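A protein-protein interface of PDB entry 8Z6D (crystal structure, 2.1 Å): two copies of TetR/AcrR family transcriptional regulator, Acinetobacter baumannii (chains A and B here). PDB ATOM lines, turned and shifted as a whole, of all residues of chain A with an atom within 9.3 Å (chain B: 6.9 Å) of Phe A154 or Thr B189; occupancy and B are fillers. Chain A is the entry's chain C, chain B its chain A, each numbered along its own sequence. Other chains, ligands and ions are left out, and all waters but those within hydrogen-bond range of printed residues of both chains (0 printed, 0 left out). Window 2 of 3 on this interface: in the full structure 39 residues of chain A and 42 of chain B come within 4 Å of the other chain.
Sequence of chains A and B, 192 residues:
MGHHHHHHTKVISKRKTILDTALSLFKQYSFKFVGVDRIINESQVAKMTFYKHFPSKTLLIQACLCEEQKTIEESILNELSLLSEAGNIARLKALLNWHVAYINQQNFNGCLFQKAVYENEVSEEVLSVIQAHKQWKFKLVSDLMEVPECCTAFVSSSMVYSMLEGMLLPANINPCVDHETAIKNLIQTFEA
The side-chain hydroxyl (OG1) of Thr B189 sits at hydrogen-bond distance from the backbone carbonyl oxygen (O) of Leu B186 (2.8 Å).
The side-chain hydroxyl (OG) of Ser A156 lies close to the backbone NH (N) of Met A159 (3.2 Å).
The backbone carbonyl oxygen (O) of Leu A186 sits at hydrogen-bond distance from the side-chain hydroxyl (OG1) of Thr A189 (3.0 Å).
Among the printed residues, merely in contact across the chains: Phe A154 with Thr B189, Val A155 with Val B155, Met A159 with Leu B186 and Thr A189 with Phe B154.
Of chain B, only Thr B189 (3.6 Å) comes within 4 Å of Phe A154.
Of the printed residues of chain B, Val A155 touches Val B155.
Printed residues of chain B within 4 Å of Met A159: Leu B186.
Printed residues of chain A within 4 Å of Phe B154: Thr A189.
Met A145 touches none of the printed residues of chain B.
The nearest printed residue of chain A that does not touch Phe B154 is Phe A154 (5.4 Å).
Hydrophobic or aromatic side chains of chain A that line the printed part of chain B: Val A155 and Met A159.
Of the 12 printed residues of chain B, 4 touch a printed residue of chain A.
Hydrophobic or aromatic side chains of chain B that line the printed part of chain A: Val B155 and Leu B186.
Among the printed residues, no Asp or Glu carboxylate lies within 4 Å of a Lys or Arg side-chain nitrogen of the other chain.
Phe A154 touches Thr B189, and with the chains exchanged Thr A189 touches Phe B154.
Val A155 touches its own counterpart, Val B155.
Positions printed for both chains: 154, 155, 186, 189 and 190.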
ATOM      1  N   MET A 145      12.527 -12.721 -22.486  1.00  0.00           N
ATOM      2  CA  MET A 145      12.418 -14.018 -23.136  1.00  0.00           C
ATOM      3  C   MET A 145      11.132 -14.181 -23.947  1.00  0.00           C
ATOM      4  O   MET A 145      11.046 -15.118 -24.747  1.00  0.00           O
ATOM      5  CB  MET A 145      12.518 -15.122 -22.085  1.00  0.00           C
ATOM      6  CG  MET A 145      13.737 -14.977 -21.183  1.00  0.00           C
ATOM      7  SD  MET A 145      14.209 -16.498 -20.318  1.00  0.00           S
ATOM      8  CE  MET A 145      13.343 -17.712 -21.321  1.00  0.00           C
ATOM      9  N   CYS A 150      13.649 -16.300 -29.194  1.00  0.00           N
ATOM     10  CA  CYS A 150      13.945 -17.233 -28.110  1.00  0.00           C
ATOM     11  C   CYS A 150      13.296 -18.599 -28.373  1.00  0.00           C
ATOM     12  O   CYS A 150      12.741 -19.233 -27.472  1.00  0.00           O
ATOM     13  CB  CYS A 150      13.469 -16.649 -26.777  1.00  0.00           C
ATOM     14  SG  CYS A 150      14.533 -16.977 -25.338  1.00  0.00           S
ATOM     15  N   ALA A 153      12.840 -21.346 -25.870  1.00  0.00           N
ATOM     16  CA  ALA A 153      13.509 -22.638 -26.003  1.00  0.00           C
ATOM     17  C   ALA A 153      12.925 -23.655 -25.005  1.00  0.00           C
ATOM     18  O   ALA A 153      11.762 -23.536 -24.603  1.00  0.00           O
ATOM     19  CB  ALA A 153      15.017 -22.478 -25.808  1.00  0.00           C
ATOM     20  N   PHE A 154      13.716 -24.667 -24.628  1.00  0.00           N
ATOM     21  CA  PHE A 154      13.292 -25.656 -23.632  1.00  0.00           C
ATOM     22  C   PHE A 154      13.422 -25.132 -22.208  1.00  0.00           C
ATOM     23  O   PHE A 154      13.276 -25.899 -21.243  1.00  0.00           O
ATOM     24  CB  PHE A 154      14.099 -26.951 -23.784  1.00  0.00           C
ATOM     25  N   VAL A 155      13.680 -23.838 -22.066  1.00  0.00           N
ATOM     26  CA  VAL A 155      13.905 -23.202 -20.779  1.00  0.00           C
ATOM     27  C   VAL A 155      12.873 -22.096 -20.631  1.00  0.00           C
ATOM     28  O   VAL A 155      12.775 -21.214 -21.493  1.00  0.00           O
ATOM     29  CB  VAL A 155      15.330 -22.645 -20.673  1.00  0.00           C
ATOM     30  CG1 VAL A 155      15.460 -21.827 -19.432  1.00  0.00           C
ATOM     31  CG2 VAL A 155      16.347 -23.782 -20.687  1.00  0.00           C
ATOM     32  N   SER A 156      12.097 -22.144 -19.557  1.00  0.00           N
ATOM     33  CA  SER A 156      11.098 -21.111 -19.349  1.00  0.00           C
ATOM     34  C   SER A 156      11.717 -19.926 -18.620  1.00  0.00           C
ATOM     35  O   SER A 156      12.799 -20.022 -18.038  1.00  0.00           O
ATOM     36  CB  SER A 156       9.895 -21.665 -18.579  1.00  0.00           C
ATOM     37  OG  SER A 156      10.122 -21.773 -17.184  1.00  0.00           O
ATOM     38  N   SER A 157      11.017 -18.791 -18.675  1.00  0.00           N
ATOM     39  CA  SER A 157      11.474 -17.602 -17.963  1.00  0.00           C
ATOM     40  C   SER A 157      11.427 -17.803 -16.458  1.00  0.00           C
ATOM     41  O   SER A 157      12.237 -17.215 -15.726  1.00  0.00           O
ATOM     42  CB  SER A 157      10.635 -16.394 -18.365  1.00  0.00           C
ATOM     43  OG  SER A 157       9.255 -16.707 -18.336  1.00  0.00           O
ATOM     44  N   MET A 159      12.154 -20.605 -14.933  1.00  0.00           N
ATOM     45  CA  MET A 159      13.421 -21.295 -14.697  1.00  0.00           C
ATOM     46  C   MET A 159      14.607 -20.330 -14.724  1.00  0.00           C
ATOM     47  O   MET A 159      15.525 -20.437 -13.901  1.00  0.00           O
ATOM     48  CB  MET A 159      13.623 -22.392 -15.752  1.00  0.00           C
ATOM     49  CG  MET A 159      12.424 -23.334 -15.967  1.00  0.00           C
ATOM     50  SD  MET A 159      12.843 -24.748 -17.029  1.00  0.00           S
ATOM     51  CE  MET A 159      14.641 -24.633 -16.996  1.00  0.00           C
ATOM     52  N   VAL A 160      14.621 -19.401 -15.677  1.00  0.00           N
ATOM     53  CA  VAL A 160      15.742 -18.464 -15.776  1.00  0.00           C
ATOM     54  C   VAL A 160      15.772 -17.533 -14.561  1.00  0.00           C
ATOM     55  O   VAL A 160      16.822 -17.368 -13.920  1.00  0.00           O
ATOM     56  CB  VAL A 160      15.677 -17.702 -17.116  1.00  0.00           C
ATOM     57  CG1 VAL A 160      16.622 -16.492 -17.139  1.00  0.00           C
ATOM     58  CG2 VAL A 160      16.043 -18.635 -18.241  1.00  0.00           C
ATOM     59  N   LEU A 186      24.748 -20.781 -21.032  1.00  0.00           N
ATOM     60  CA  LEU A 186      23.352 -20.424 -21.248  1.00  0.00           C
ATOM     61  C   LEU A 186      23.210 -19.349 -22.325  1.00  0.00           C
ATOM     62  O   LEU A 186      22.278 -19.395 -23.137  1.00  0.00           O
ATOM     63  CB  LEU A 186      22.721 -19.965 -19.938  1.00  0.00           C
ATOM     64  CG  LEU A 186      21.297 -19.434 -20.092  1.00  0.00           C
ATOM     65  CD1 LEU A 186      20.388 -20.522 -20.627  1.00  0.00           C
ATOM     66  CD2 LEU A 186      20.782 -18.907 -18.776  1.00  0.00           C
ATOM     67  N   THR A 189      23.453 -21.195 -25.589  1.00  0.00           N
ATOM     68  CA  THR A 189      22.242 -21.909 -25.984  1.00  0.00           C
ATOM     69  C   THR A 189      21.216 -20.969 -26.617  1.00  0.00           C
ATOM     70  O   THR A 189      20.489 -21.382 -27.529  1.00  0.00           O
ATOM     71  CB  THR A 189      21.618 -22.652 -24.797  1.00  0.00           C
ATOM     72  OG1 THR A 189      20.749 -21.771 -24.070  1.00  0.00           O
ATOM     73  CG2 THR A 189      22.680 -23.244 -23.868  1.00  0.00           C
ATOM     74  N   PHE A 190      21.147 -19.709 -26.169  1.00  0.00           N
ATOM     75  CA  PHE A 190      20.258 -18.728 -26.793  1.00  0.00           C
ATOM     76  C   PHE A 190      20.772 -18.220 -28.136  1.00  0.00           C
ATOM     77  O   PHE A 190      20.067 -17.431 -28.777  1.00  0.00           O
ATOM     78  CB  PHE A 190      20.033 -17.543 -25.854  1.00  0.00           C
ATOM     79  CG  PHE A 190      19.128 -17.855 -24.703  1.00  0.00           C
ATOM     80  CD1 PHE A 190      18.011 -18.663 -24.880  1.00  0.00           C
ATOM     81  CD2 PHE A 190      19.397 -17.353 -23.442  1.00  0.00           C
ATOM     82  CE1 PHE A 190      17.177 -18.964 -23.821  1.00  0.00           C
ATOM     83  CE2 PHE A 190      18.567 -17.647 -22.374  1.00  0.00           C
ATOM     84  CZ  PHE A 190      17.456 -18.457 -22.560  1.00  0.00           C
ATOM     85  N   CYS B 151      20.424 -33.886 -22.319  1.00  0.00           N
ATOM     86  CA  CYS B 151      21.153 -32.945 -23.181  1.00  0.00           C
ATOM     87  C   CYS B 151      22.144 -32.093 -22.383  1.00  0.00           C
ATOM     88  O   CYS B 151      21.966 -30.880 -22.232  1.00  0.00           O
ATOM     89  CB  CYS B 151      20.178 -32.026 -23.936  1.00  0.00           C
ATOM     90  SG  CYS B 151      18.546 -31.811 -23.159  1.00  0.00           S
ATOM     91  N   PHE B 154      21.706 -28.769 -24.180  1.00  0.00           N
ATOM     92  CA  PHE B 154      20.600 -27.829 -24.033  1.00  0.00           C
ATOM     93  C   PHE B 154      20.660 -27.114 -22.685  1.00  0.00           C
ATOM     94  O   PHE B 154      21.128 -25.977 -22.595  1.00  0.00           O
ATOM     95  CB  PHE B 154      19.256 -28.547 -24.180  1.00  0.00           C
ATOM     96  N   VAL B 155      20.177 -27.780 -21.638  1.00  0.00           N
ATOM     97  CA  VAL B 155      20.160 -27.236 -20.282  1.00  0.00           C
ATOM     98  C   VAL B 155      21.281 -27.894 -19.494  1.00  0.00           C
ATOM     99  O   VAL B 155      21.345 -29.126 -19.424  1.00  0.00           O
ATOM    100  CB  VAL B 155      18.803 -27.487 -19.603  1.00  0.00           C
ATOM    101  CG1 VAL B 155      18.583 -26.494 -18.498  1.00  0.00           C
ATOM    102  CG2 VAL B 155      17.674 -27.434 -20.626  1.00  0.00           C
ATOM    103  N   LYS B 184       7.296 -28.771 -13.110  1.00  0.00           N
ATOM    104  CA  LYS B 184       6.496 -29.666 -13.946  1.00  0.00           C
ATOM    105  C   LYS B 184       6.786 -29.439 -15.426  1.00  0.00           C
ATOM    106  O   LYS B 184       6.822 -30.390 -16.214  1.00  0.00           O
ATOM    107  CB  LYS B 184       5.002 -29.482 -13.667  1.00  0.00           C
ATOM    108  CG  LYS B 184       4.521 -30.083 -12.354  1.00  0.00           C
ATOM    109  N   ASN B 185       7.010 -28.183 -15.816  1.00  0.00           N
ATOM    110  CA  ASN B 185       7.308 -27.871 -17.211  1.00  0.00           C
ATOM    111  C   ASN B 185       8.676 -28.396 -17.630  1.00  0.00           C
ATOM    112  O   ASN B 185       8.830 -28.912 -18.742  1.00  0.00           O
ATOM    113  CB  ASN B 185       7.217 -26.359 -17.440  1.00  0.00           C
ATOM    114  CG  ASN B 185       5.775 -25.855 -17.444  1.00  0.00           C
ATOM    115  OD1 ASN B 185       4.831 -26.636 -17.620  1.00  0.00           O
ATOM    116  ND2 ASN B 185       5.599 -24.551 -17.226  1.00  0.00           N
ATOM    117  N   LEU B 186       9.684 -28.271 -16.766  1.00  0.00           N
ATOM    118  CA  LEU B 186      11.011 -28.764 -17.131  1.00  0.00           C
ATOM    119  C   LEU B 186      11.060 -30.289 -17.161  1.00  0.00           C
ATOM    120  O   LEU B 186      11.837 -30.867 -17.936  1.00  0.00           O
ATOM    121  CB  LEU B 186      12.066 -28.204 -16.177  1.00  0.00           C
ATOM    122  CG  LEU B 186      13.409 -28.934 -16.128  1.00  0.00           C
ATOM    123  CD1 LEU B 186      14.303 -28.437 -17.246  1.00  0.00           C
ATOM    124  CD2 LEU B 186      14.086 -28.699 -14.794  1.00  0.00           C
ATOM    125  N   ILE B 187      10.235 -30.958 -16.344  1.00  0.00           N
ATOM    126  CA  ILE B 187      10.165 -32.417 -16.402  1.00  0.00           C
ATOM    127  C   ILE B 187       9.707 -32.877 -17.785  1.00  0.00           C
ATOM    128  O   ILE B 187      10.201 -33.881 -18.311  1.00  0.00           O
ATOM    129  CB  ILE B 187       9.264 -32.959 -15.274  1.00  0.00           C
ATOM    130  CG1 ILE B 187      10.058 -33.000 -13.961  1.00  0.00           C
ATOM    131  CG2 ILE B 187       8.730 -34.345 -15.604  1.00  0.00           C
ATOM    132  CD1 ILE B 187       9.246 -33.421 -12.739  1.00  0.00           C
ATOM    133  N   GLN B 188       8.789 -32.135 -18.411  1.00  0.00           N
ATOM    134  CA  GLN B 188       8.300 -32.533 -19.730  1.00  0.00           C
ATOM    135  C   GLN B 188       9.367 -32.376 -20.808  1.00  0.00           C
ATOM    136  O   GLN B 188       9.353 -33.117 -21.798  1.00  0.00           O
ATOM    137  CB  GLN B 188       7.059 -31.732 -20.108  1.00  0.00           C
ATOM    138  CG  GLN B 188       5.797 -32.198 -19.416  1.00  0.00           C
ATOM    139  CD  GLN B 188       4.791 -31.083 -19.257  1.00  0.00           C
ATOM    140  OE1 GLN B 188       5.152 -29.907 -19.271  1.00  0.00           O
ATOM    141  NE2 GLN B 188       3.518 -31.443 -19.128  1.00  0.00           N
ATOM    142  N   THR B 189      10.298 -31.434 -20.637  1.00  0.00           N
ATOM    143  CA  THR B 189      11.397 -31.299 -21.591  1.00  0.00           C
ATOM    144  C   THR B 189      12.319 -32.515 -21.550  1.00  0.00           C
ATOM    145  O   THR B 189      12.700 -33.054 -22.599  1.00  0.00           O
ATOM    146  CB  THR B 189      12.190 -30.019 -21.315  1.00  0.00           C
ATOM    147  OG1 THR B 189      13.173 -30.280 -20.306  1.00  0.00           O
ATOM    148  CG2 THR B 189      11.270 -28.899 -20.848  1.00  0.00           C
ATOM    149  N   PHE B 190      12.698 -32.960 -20.345  1.00  0.00           N
ATOM    150  CA  PHE B 190      13.508 -34.171 -20.238  1.00  0.00           C
ATOM    151  C   PHE B 190      12.788 -35.375 -20.822  1.00  0.00           C
ATOM    152  O   PHE B 190      13.433 -36.328 -21.275  1.00  0.00           O
ATOM    153  CB  PHE B 190      13.884 -34.435 -18.783  1.00  0.00           C
ATOM    154  CG  PHE B 190      14.854 -33.446 -18.244  1.00  0.00           C
ATOM    155  CD1 PHE B 190      14.668 -32.875 -16.996  1.00  0.00           C
ATOM    156  CD2 PHE B 190      15.941 -33.049 -19.007  1.00  0.00           C
ATOM    157  CE1 PHE B 190      15.564 -31.944 -16.503  1.00  0.00           C
ATOM    158  CE2 PHE B 190      16.847 -32.118 -18.517  1.00  0.00           C
ATOM    159  CZ  PHE B 190      16.651 -31.556 -17.266  1.00  0.00           C
ATOM    160  N   GLU B 191      11.457 -35.349 -20.827  1.00  0.00           N
ATOM    161  CA  GLU B 191      10.661 -36.452 -21.343  1.00  0.00           C
ATOM    162  C   GLU B 191      10.274 -36.267 -22.793  1.00  0.00           C
ATOM    163  O   GLU B 191       9.237 -36.790 -23.223  1.00  0.00           O
ATOM    164  CB  GLU B 191       9.413 -36.630 -20.487  1.00  0.00           C
ATOM    165  CG  GLU B 191       9.643 -37.485 -19.280  1.00  0.00           C
ATOM    166  CD  GLU B 191       8.587 -37.259 -18.230  1.00  0.00           C
ATOM    167  OE1 GLU B 191       7.651 -36.467 -18.485  1.00  0.00           O
ATOM    168  OE2 GLU B 191       8.695 -37.876 -17.156  1.00  0.00           O
ATOM    169  N   ALA B 192      11.070 -35.531 -23.560  1.00  0.00           N
ATOM    170  CA  ALA B 192      10.776 -35.333 -24.976  1.00  0.00           C
ATOM    171  C   ALA B 192      11.477 -36.388 -25.825  1.00  0.00           C
ATOM    172  O   ALA B 192      10.827 -37.159 -26.534  1.00  0.00           O
ATOM    173  CB  ALA B 192      11.183 -33.939 -25.415  1.00  0.00           C
